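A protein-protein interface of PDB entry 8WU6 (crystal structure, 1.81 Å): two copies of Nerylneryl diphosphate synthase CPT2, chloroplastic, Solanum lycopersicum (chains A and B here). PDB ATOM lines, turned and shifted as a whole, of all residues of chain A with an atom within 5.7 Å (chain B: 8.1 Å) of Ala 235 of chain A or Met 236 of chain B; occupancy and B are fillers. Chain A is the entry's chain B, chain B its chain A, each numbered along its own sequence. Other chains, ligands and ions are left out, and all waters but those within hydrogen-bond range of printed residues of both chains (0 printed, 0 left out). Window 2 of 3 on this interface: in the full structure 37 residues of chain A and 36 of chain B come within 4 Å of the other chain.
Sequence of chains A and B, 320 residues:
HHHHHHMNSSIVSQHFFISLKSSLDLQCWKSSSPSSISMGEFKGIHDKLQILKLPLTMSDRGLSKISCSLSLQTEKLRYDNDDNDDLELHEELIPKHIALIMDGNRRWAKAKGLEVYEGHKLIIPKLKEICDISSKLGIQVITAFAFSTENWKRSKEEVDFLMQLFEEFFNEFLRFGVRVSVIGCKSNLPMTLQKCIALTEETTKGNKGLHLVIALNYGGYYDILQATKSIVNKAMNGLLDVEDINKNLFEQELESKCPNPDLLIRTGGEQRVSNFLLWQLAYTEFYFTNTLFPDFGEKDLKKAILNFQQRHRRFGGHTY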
ATOM      1  N   SER A 230     -31.334  -8.978  20.192  1.00  0.00           N
ATOM      2  CA  SER A 230     -30.905 -10.377  20.122  1.00  0.00           C
ATOM      3  C   SER A 230     -29.394 -10.487  19.978  1.00  0.00           C
ATOM      4  O   SER A 230     -28.763 -11.332  20.634  1.00  0.00           O
ATOM      5  CB  SER A 230     -31.577 -11.086  18.952  1.00  0.00           C
ATOM      6  OG  SER A 230     -31.164 -12.441  18.894  1.00  0.00           O
ATOM      7  N   ILE A 231     -28.806  -9.654  19.105  1.00  0.00           N
ATOM      8  CA  ILE A 231     -27.356  -9.657  18.902  1.00  0.00           C
ATOM      9  C   ILE A 231     -26.634  -9.192  20.156  1.00  0.00           C
ATOM     10  O   ILE A 231     -25.626  -9.795  20.565  1.00  0.00           O
ATOM     11  CB  ILE A 231     -26.994  -8.791  17.682  1.00  0.00           C
ATOM     12  CG1 ILE A 231     -27.490  -9.489  16.415  1.00  0.00           C
ATOM     13  CG2 ILE A 231     -25.469  -8.564  17.608  1.00  0.00           C
ATOM     14  CD1 ILE A 231     -27.494  -8.594  15.143  1.00  0.00           C
ATOM     15  N   VAL A 232     -27.135  -8.136  20.801  1.00  0.00           N
ATOM     16  CA  VAL A 232     -26.540  -7.715  22.078  1.00  0.00           C
ATOM     17  C   VAL A 232     -26.587  -8.855  23.087  1.00  0.00           C
ATOM     18  O   VAL A 232     -25.606  -9.126  23.795  1.00  0.00           O
ATOM     19  CB  VAL A 232     -27.253  -6.464  22.631  1.00  0.00           C
ATOM     20  CG1 VAL A 232     -26.753  -6.152  24.078  1.00  0.00           C
ATOM     21  CG2 VAL A 232     -27.064  -5.252  21.704  1.00  0.00           C
ATOM     22  N   ASN A 233     -27.729  -9.538  23.186  1.00  0.00           N
ATOM     23  CA  ASN A 233     -27.836 -10.609  24.180  1.00  0.00           C
ATOM     24  C   ASN A 233     -26.836 -11.725  23.908  1.00  0.00           C
ATOM     25  O   ASN A 233     -26.216 -12.258  24.840  1.00  0.00           O
ATOM     26  CB  ASN A 233     -29.259 -11.163  24.216  1.00  0.00           C
ATOM     27  CG  ASN A 233     -30.166 -10.367  25.127  1.00  0.00           C
ATOM     28  OD1 ASN A 233     -29.739  -9.870  26.181  1.00  0.00           O
ATOM     29  ND2 ASN A 233     -31.421 -10.220  24.721  1.00  0.00           N
ATOM     30  N   LYS A 234     -26.673 -12.099  22.638  1.00  0.00           N
ATOM     31  CA  LYS A 234     -25.710 -13.141  22.307  1.00  0.00           C
ATOM     32  C   LYS A 234     -24.300 -12.704  22.652  1.00  0.00           C
ATOM     33  O   LYS A 234     -23.514 -13.490  23.205  1.00  0.00           O
ATOM     34  CB  LYS A 234     -25.832 -13.495  20.831  1.00  0.00           C
ATOM     35  CG  LYS A 234     -27.128 -14.247  20.538  1.00  0.00           C
ATOM     36  CD  LYS A 234     -27.247 -14.560  19.071  1.00  0.00           C
ATOM     37  CE  LYS A 234     -28.543 -15.316  18.801  1.00  0.00           C
ATOM     38  NZ  LYS A 234     -28.666 -15.598  17.358  1.00  0.00           N
ATOM     39  N   ALA A 235     -23.960 -11.442  22.352  1.00  0.00           N
ATOM     40  CA  ALA A 235     -22.628 -10.943  22.696  1.00  0.00           C
ATOM     41  C   ALA A 235     -22.395 -10.959  24.200  1.00  0.00           C
ATOM     42  O   ALA A 235     -21.309 -11.328  24.667  1.00  0.00           O
ATOM     43  CB  ALA A 235     -22.434  -9.518  22.165  1.00  0.00           C
ATOM     44  N   MET A 236     -23.399 -10.537  24.970  1.00  0.00           N
ATOM     45  CA  MET A 236     -23.267 -10.450  26.425  1.00  0.00           C
ATOM     46  C   MET A 236     -23.219 -11.822  27.076  1.00  0.00           C
ATOM     47  O   MET A 236     -22.652 -11.972  28.166  1.00  0.00           O
ATOM     48  CB  MET A 236     -24.434  -9.608  26.942  1.00  0.00           C
ATOM     49  CG  MET A 236     -24.148  -8.096  26.843  1.00  0.00           C
ATOM     50  SD  MET A 236     -25.591  -7.113  27.318  1.00  0.00           S
ATOM     51  CE  MET A 236     -25.023  -6.757  28.986  1.00  0.00           C
ATOM     52  N   ASN A 237     -23.757 -12.837  26.414  1.00  0.00           N
ATOM     53  CA  ASN A 237     -23.736 -14.185  26.945  1.00  0.00           C
ATOM     54  C   ASN A 237     -22.539 -14.992  26.458  1.00  0.00           C
ATOM     55  O   ASN A 237     -22.426 -16.173  26.801  1.00  0.00           O
ATOM     56  CB  ASN A 237     -25.047 -14.898  26.609  1.00  0.00           C
ATOM     57  CG  ASN A 237     -26.201 -14.404  27.473  1.00  0.00           C
ATOM     58  OD1 ASN A 237     -26.027 -14.181  28.672  1.00  0.00           O
ATOM     59  ND2 ASN A 237     -27.380 -14.243  26.876  1.00  0.00           N
ATOM     60  N   GLY A 238     -21.601 -14.354  25.756  1.00  0.00           N
ATOM     61  CA  GLY A 238     -20.384 -15.007  25.290  1.00  0.00           C
ATOM     62  C   GLY A 238     -20.551 -15.868  24.059  1.00  0.00           C
ATOM     63  O   GLY A 238     -19.613 -16.582  23.683  1.00  0.00           O
ATOM     64  N   LEU A 239     -21.673 -15.747  23.352  1.00  0.00           N
ATOM     65  CA  LEU A 239     -21.950 -16.620  22.226  1.00  0.00           C
ATOM     66  C   LEU A 239     -21.495 -16.045  20.906  1.00  0.00           C
ATOM     67  O   LEU A 239     -21.609 -16.731  19.886  1.00  0.00           O
ATOM     68  CB  LEU A 239     -23.452 -16.902  22.121  1.00  0.00           C
ATOM     69  CG  LEU A 239     -24.087 -17.638  23.279  1.00  0.00           C
ATOM     70  CD1 LEU A 239     -25.588 -17.681  23.026  1.00  0.00           C
ATOM     71  CD2 LEU A 239     -23.488 -19.044  23.378  1.00  0.00           C
ATOM     72  N   LEU A 240     -20.954 -14.831  20.890  1.00  0.00           N
ATOM     73  CA  LEU A 240     -20.668 -14.171  19.633  1.00  0.00           C
ATOM     74  C   LEU A 240     -19.347 -13.421  19.693  1.00  0.00           C
ATOM     75  O   LEU A 240     -19.074 -12.683  20.648  1.00  0.00           O
ATOM     76  CB  LEU A 240     -21.828 -13.189  19.322  1.00  0.00           C
ATOM     77  CG  LEU A 240     -21.821 -12.262  18.115  1.00  0.00           C
ATOM     78  CD1 LEU A 240     -21.921 -13.061  16.828  1.00  0.00           C
ATOM     79  CD2 LEU A 240     -23.008 -11.290  18.232  1.00  0.00           C
ATOM     80  N   VAL A 242     -17.577 -10.319  18.312  1.00  0.00           N
ATOM     81  CA  VAL A 242     -18.117  -9.078  17.743  1.00  0.00           C
ATOM     82  C   VAL A 242     -17.645  -8.852  16.317  1.00  0.00           C
ATOM     83  O   VAL A 242     -18.308  -8.147  15.552  1.00  0.00           O
ATOM     84  CB  VAL A 242     -17.806  -7.860  18.637  1.00  0.00           C
ATOM     85  CG1 VAL A 242     -18.589  -7.970  19.946  1.00  0.00           C
ATOM     86  CG2 VAL A 242     -16.298  -7.707  18.870  1.00  0.00           C
ATOM     87  N   LYS B 229     -23.350  -2.214  15.848  1.00  0.00           N
ATOM     88  CA  LYS B 229     -22.028  -2.521  16.407  1.00  0.00           C
ATOM     89  C   LYS B 229     -21.679  -1.595  17.559  1.00  0.00           C
ATOM     90  O   LYS B 229     -21.059  -2.024  18.547  1.00  0.00           O
ATOM     91  CB  LYS B 229     -20.955  -2.422  15.322  1.00  0.00           C
ATOM     92  CG  LYS B 229     -21.021  -3.564  14.311  1.00  0.00           C
ATOM     93  CD  LYS B 229     -20.026  -3.284  13.162  1.00  0.00           C
ATOM     94  CE  LYS B 229     -20.182  -4.269  12.018  1.00  0.00           C
ATOM     95  NZ  LYS B 229     -19.313  -3.898  10.849  1.00  0.00           N
ATOM     96  N   SER B 230     -22.017  -0.308  17.419  1.00  0.00           N
ATOM     97  CA  SER B 230     -21.784   0.660  18.477  1.00  0.00           C
ATOM     98  C   SER B 230     -22.558   0.307  19.747  1.00  0.00           C
ATOM     99  O   SER B 230     -22.024   0.396  20.866  1.00  0.00           O
ATOM    100  CB  SER B 230     -22.170   2.050  17.975  1.00  0.00           C
ATOM    101  OG  SER B 230     -21.946   3.004  19.002  1.00  0.00           O
ATOM    102  N   ILE B 231     -23.814  -0.090  19.589  1.00  0.00           N
ATOM    103  CA  ILE B 231     -24.651  -0.443  20.725  1.00  0.00           C
ATOM    104  C   ILE B 231     -24.120  -1.696  21.410  1.00  0.00           C
ATOM    105  O   ILE B 231     -24.053  -1.759  22.646  1.00  0.00           O
ATOM    106  CB  ILE B 231     -26.099  -0.598  20.248  1.00  0.00           C
ATOM    107  CG1 ILE B 231     -26.662   0.793  19.933  1.00  0.00           C
ATOM    108  CG2 ILE B 231     -26.938  -1.367  21.276  1.00  0.00           C
ATOM    109  CD1 ILE B 231     -27.957   0.748  19.148  1.00  0.00           C
ATOM    110  N   VAL B 232     -23.700  -2.692  20.621  1.00  0.00           N
ATOM    111  CA  VAL B 232     -23.073  -3.893  21.197  1.00  0.00           C
ATOM    112  C   VAL B 232     -21.841  -3.518  22.011  1.00  0.00           C
ATOM    113  O   VAL B 232     -21.656  -3.997  23.139  1.00  0.00           O
ATOM    114  CB  VAL B 232     -22.728  -4.905  20.089  1.00  0.00           C
ATOM    115  CG1 VAL B 232     -21.805  -5.999  20.634  1.00  0.00           C
ATOM    116  CG2 VAL B 232     -24.021  -5.511  19.542  1.00  0.00           C
ATOM    117  N   ASN B 233     -20.993  -2.643  21.458  1.00  0.00           N
ATOM    118  CA  ASN B 233     -19.766  -2.249  22.146  1.00  0.00           C
ATOM    119  C   ASN B 233     -20.079  -1.553  23.479  1.00  0.00           C
ATOM    120  O   ASN B 233     -19.427  -1.824  24.498  1.00  0.00           O
ATOM    121  CB  ASN B 233     -18.948  -1.333  21.237  1.00  0.00           C
ATOM    122  CG  ASN B 233     -17.724  -0.761  21.931  1.00  0.00           C
ATOM    123  OD1 ASN B 233     -17.705   0.399  22.332  1.00  0.00           O
ATOM    124  ND2 ASN B 233     -16.676  -1.566  22.026  1.00  0.00           N
ATOM    125  N   LYS B 234     -21.081  -0.669  23.489  1.00  0.00           N
ATOM    126  CA  LYS B 234     -21.464  -0.009  24.738  1.00  0.00           C
ATOM    127  C   LYS B 234     -21.980  -1.011  25.772  1.00  0.00           C
ATOM    128  O   LYS B 234     -21.585  -0.944  26.943  1.00  0.00           O
ATOM    129  CB  LYS B 234     -22.516   1.073  24.484  1.00  0.00           C
ATOM    130  CG  LYS B 234     -21.958   2.287  23.755  1.00  0.00           C
ATOM    131  CD  LYS B 234     -23.066   3.167  23.216  1.00  0.00           C
ATOM    132  CE  LYS B 234     -22.526   4.563  23.013  1.00  0.00           C
ATOM    133  NZ  LYS B 234     -21.574   4.567  21.865  1.00  0.00           N
ATOM    134  N   ALA B 235     -22.834  -1.960  25.359  1.00  0.00           N
ATOM    135  CA  ALA B 235     -23.308  -2.997  26.280  1.00  0.00           C
ATOM    136  C   ALA B 235     -22.160  -3.839  26.827  1.00  0.00           C
ATOM    137  O   ALA B 235     -22.144  -4.188  28.020  1.00  0.00           O
ATOM    138  CB  ALA B 235     -24.323  -3.917  25.578  1.00  0.00           C
ATOM    139  N   MET B 236     -21.198  -4.207  25.970  1.00  0.00           N
ATOM    140  CA  MET B 236     -20.083  -5.044  26.423  1.00  0.00           C
ATOM    141  C   MET B 236     -19.152  -4.309  27.388  1.00  0.00           C
ATOM    142  O   MET B 236     -18.443  -4.955  28.190  1.00  0.00           O
ATOM    143  CB  MET B 236     -19.289  -5.523  25.205  1.00  0.00           C
ATOM    144  CG  MET B 236     -19.989  -6.530  24.293  1.00  0.00           C
ATOM    145  SD  MET B 236     -20.644  -7.900  25.194  1.00  0.00           S
ATOM    146  CE  MET B 236     -19.168  -8.924  25.329  1.00  0.00           C
ATOM    147  N   ASN B 237     -19.140  -2.982  27.329  1.00  0.00           N
ATOM    148  CA  ASN B 237     -18.366  -2.156  28.245  1.00  0.00           C
ATOM    149  C   ASN B 237     -19.169  -1.691  29.452  1.00  0.00           C
ATOM    150  O   ASN B 237     -18.688  -0.842  30.204  1.00  0.00           O
ATOM    151  CB  ASN B 237     -17.784  -0.943  27.519  1.00  0.00           C
ATOM    152  CG  ASN B 237     -16.555  -1.293  26.696  1.00  0.00           C
ATOM    153  OD1 ASN B 237     -15.556  -1.770  27.235  1.00  0.00           O
ATOM    154  ND2 ASN B 237     -16.603  -1.025  25.418  1.00  0.00           N
ATOM    155  N   GLY B 238     -20.378  -2.212  29.657  1.00  0.00           N
ATOM    156  CA  GLY B 238     -21.131  -1.822  30.837  1.00  0.00           C
ATOM    157  C   GLY B 238     -21.768  -0.448  30.791  1.00  0.00           C
ATOM    158  O   GLY B 238     -22.093   0.100  31.851  1.00  0.00           O
ATOM    159  N   LEU B 239     -21.913   0.160  29.601  1.00  0.00           N
ATOM    160  CA  LEU B 239     -22.462   1.513  29.495  1.00  0.00           C
ATOM    161  C   LEU B 239     -23.962   1.557  29.181  1.00  0.00           C
ATOM    162  O   LEU B 239     -24.524   2.665  29.123  1.00  0.00           O
ATOM    163  CB  LEU B 239     -21.679   2.303  28.428  1.00  0.00           C
ATOM    164  CG  LEU B 239     -20.152   2.350  28.602  1.00  0.00           C
ATOM    165  CD1 LEU B 239     -19.515   3.238  27.514  1.00  0.00           C
ATOM    166  CD2 LEU B 239     -19.778   2.859  29.998  1.00  0.00           C
ATOM    167  N   LEU B 240     -24.545   0.424  28.842  1.00  0.00           N
ATOM    168  CA  LEU B 240     -26.002   0.446  28.601  1.00  0.00           C
ATOM    169  C   LEU B 240     -26.634  -0.916  28.844  1.00  0.00           C
ATOM    170  O   LEU B 240     -25.925  -1.917  28.766  1.00  0.00           O
ATOM    171  CB  LEU B 240     -26.314   0.943  27.183  1.00  0.00           C
ATOM    172  CG  LEU B 240     -25.931   0.058  25.998  1.00  0.00           C
ATOM    173  CD1 LEU B 240     -26.933  -1.066  25.801  1.00  0.00           C
ATOM    174  CD2 LEU B 240     -25.866   0.901  24.738  1.00  0.00           C
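Of the printed residues of chain B, Ile 231 of chain A touches Val 232.
Printed residues of chain B within 4 Å of Val 232 of chain A: Ile 231, Val 232 and Ala 235.
Of chain B, only Val 232 and Met 236 come within 4 Å of Ala 235 of chain A.
Of the printed residues of chain A, Ile 231 of chain B touches Val 232.
Printed residues of chain A within 4 Å of Val 232 of chain B: Ile 231, Val 232, Ala 235 and Val 242.
The nearest residue of chain B that does not touch Ala 235 of chain A is Ala 235 of chain B (6.8 Å).
Ile 231 of chain A touches Val 232 of chain B.
Val 232 of chain A touches Ile 231 of chain B (CG2 to CG2, 3.9 Å).
CG2 of Val 232 of chain A touches CG2 of Val 232 of chain B, at 3.7 Å.
Ala 235 of chain B touches Val 232 of chain A.
Val 232 of chain B touches Ala 235 of chain A.
SD of Met 236 of chain A touches CB of Ala 235 of chain B, at 3.9 Å.
N of Met 236 of chain A touches SD of Met 236 of chain B, 3.8 Å away.
CG1 of Val 242 of chain A touches CG1 of Val 232 of chain B, at 3.8 Å.
Val 232 of chain A touches its own counterpart, Val 232 of chain B.
Val 232 of chain A touches Ala 235 of chain B, and with the chains exchanged Ala 235 of chain A touches Val 232 of chain B.
Ala 235 of chain A touches Met 236 of chain B, and with the chains exchanged Met 236 of chain A touches Ala 235 of chain B.
Met 236 of chain A touches its own counterpart, Met 236 of chain B.
Of the 9 pairs that touch across the chains among the printed residues, 8 have their exchanged pair printed and touching as well.
SD of Met 236 of chain B sits close to O of Ala 235 of chain A, at 3.5 Å.
Hydrophobic or aromatic side chains of chain A that line the printed part of chain B: Ile 231, Val 232, Ala 235, Met 236 and Val 242.
Among the printed residues, 9 pairs touch across the chains.
Among the printed residues, no Asp or Glu carboxylate lies within 4 Å of a Lys or Arg side-chain nitrogen of the other chain.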
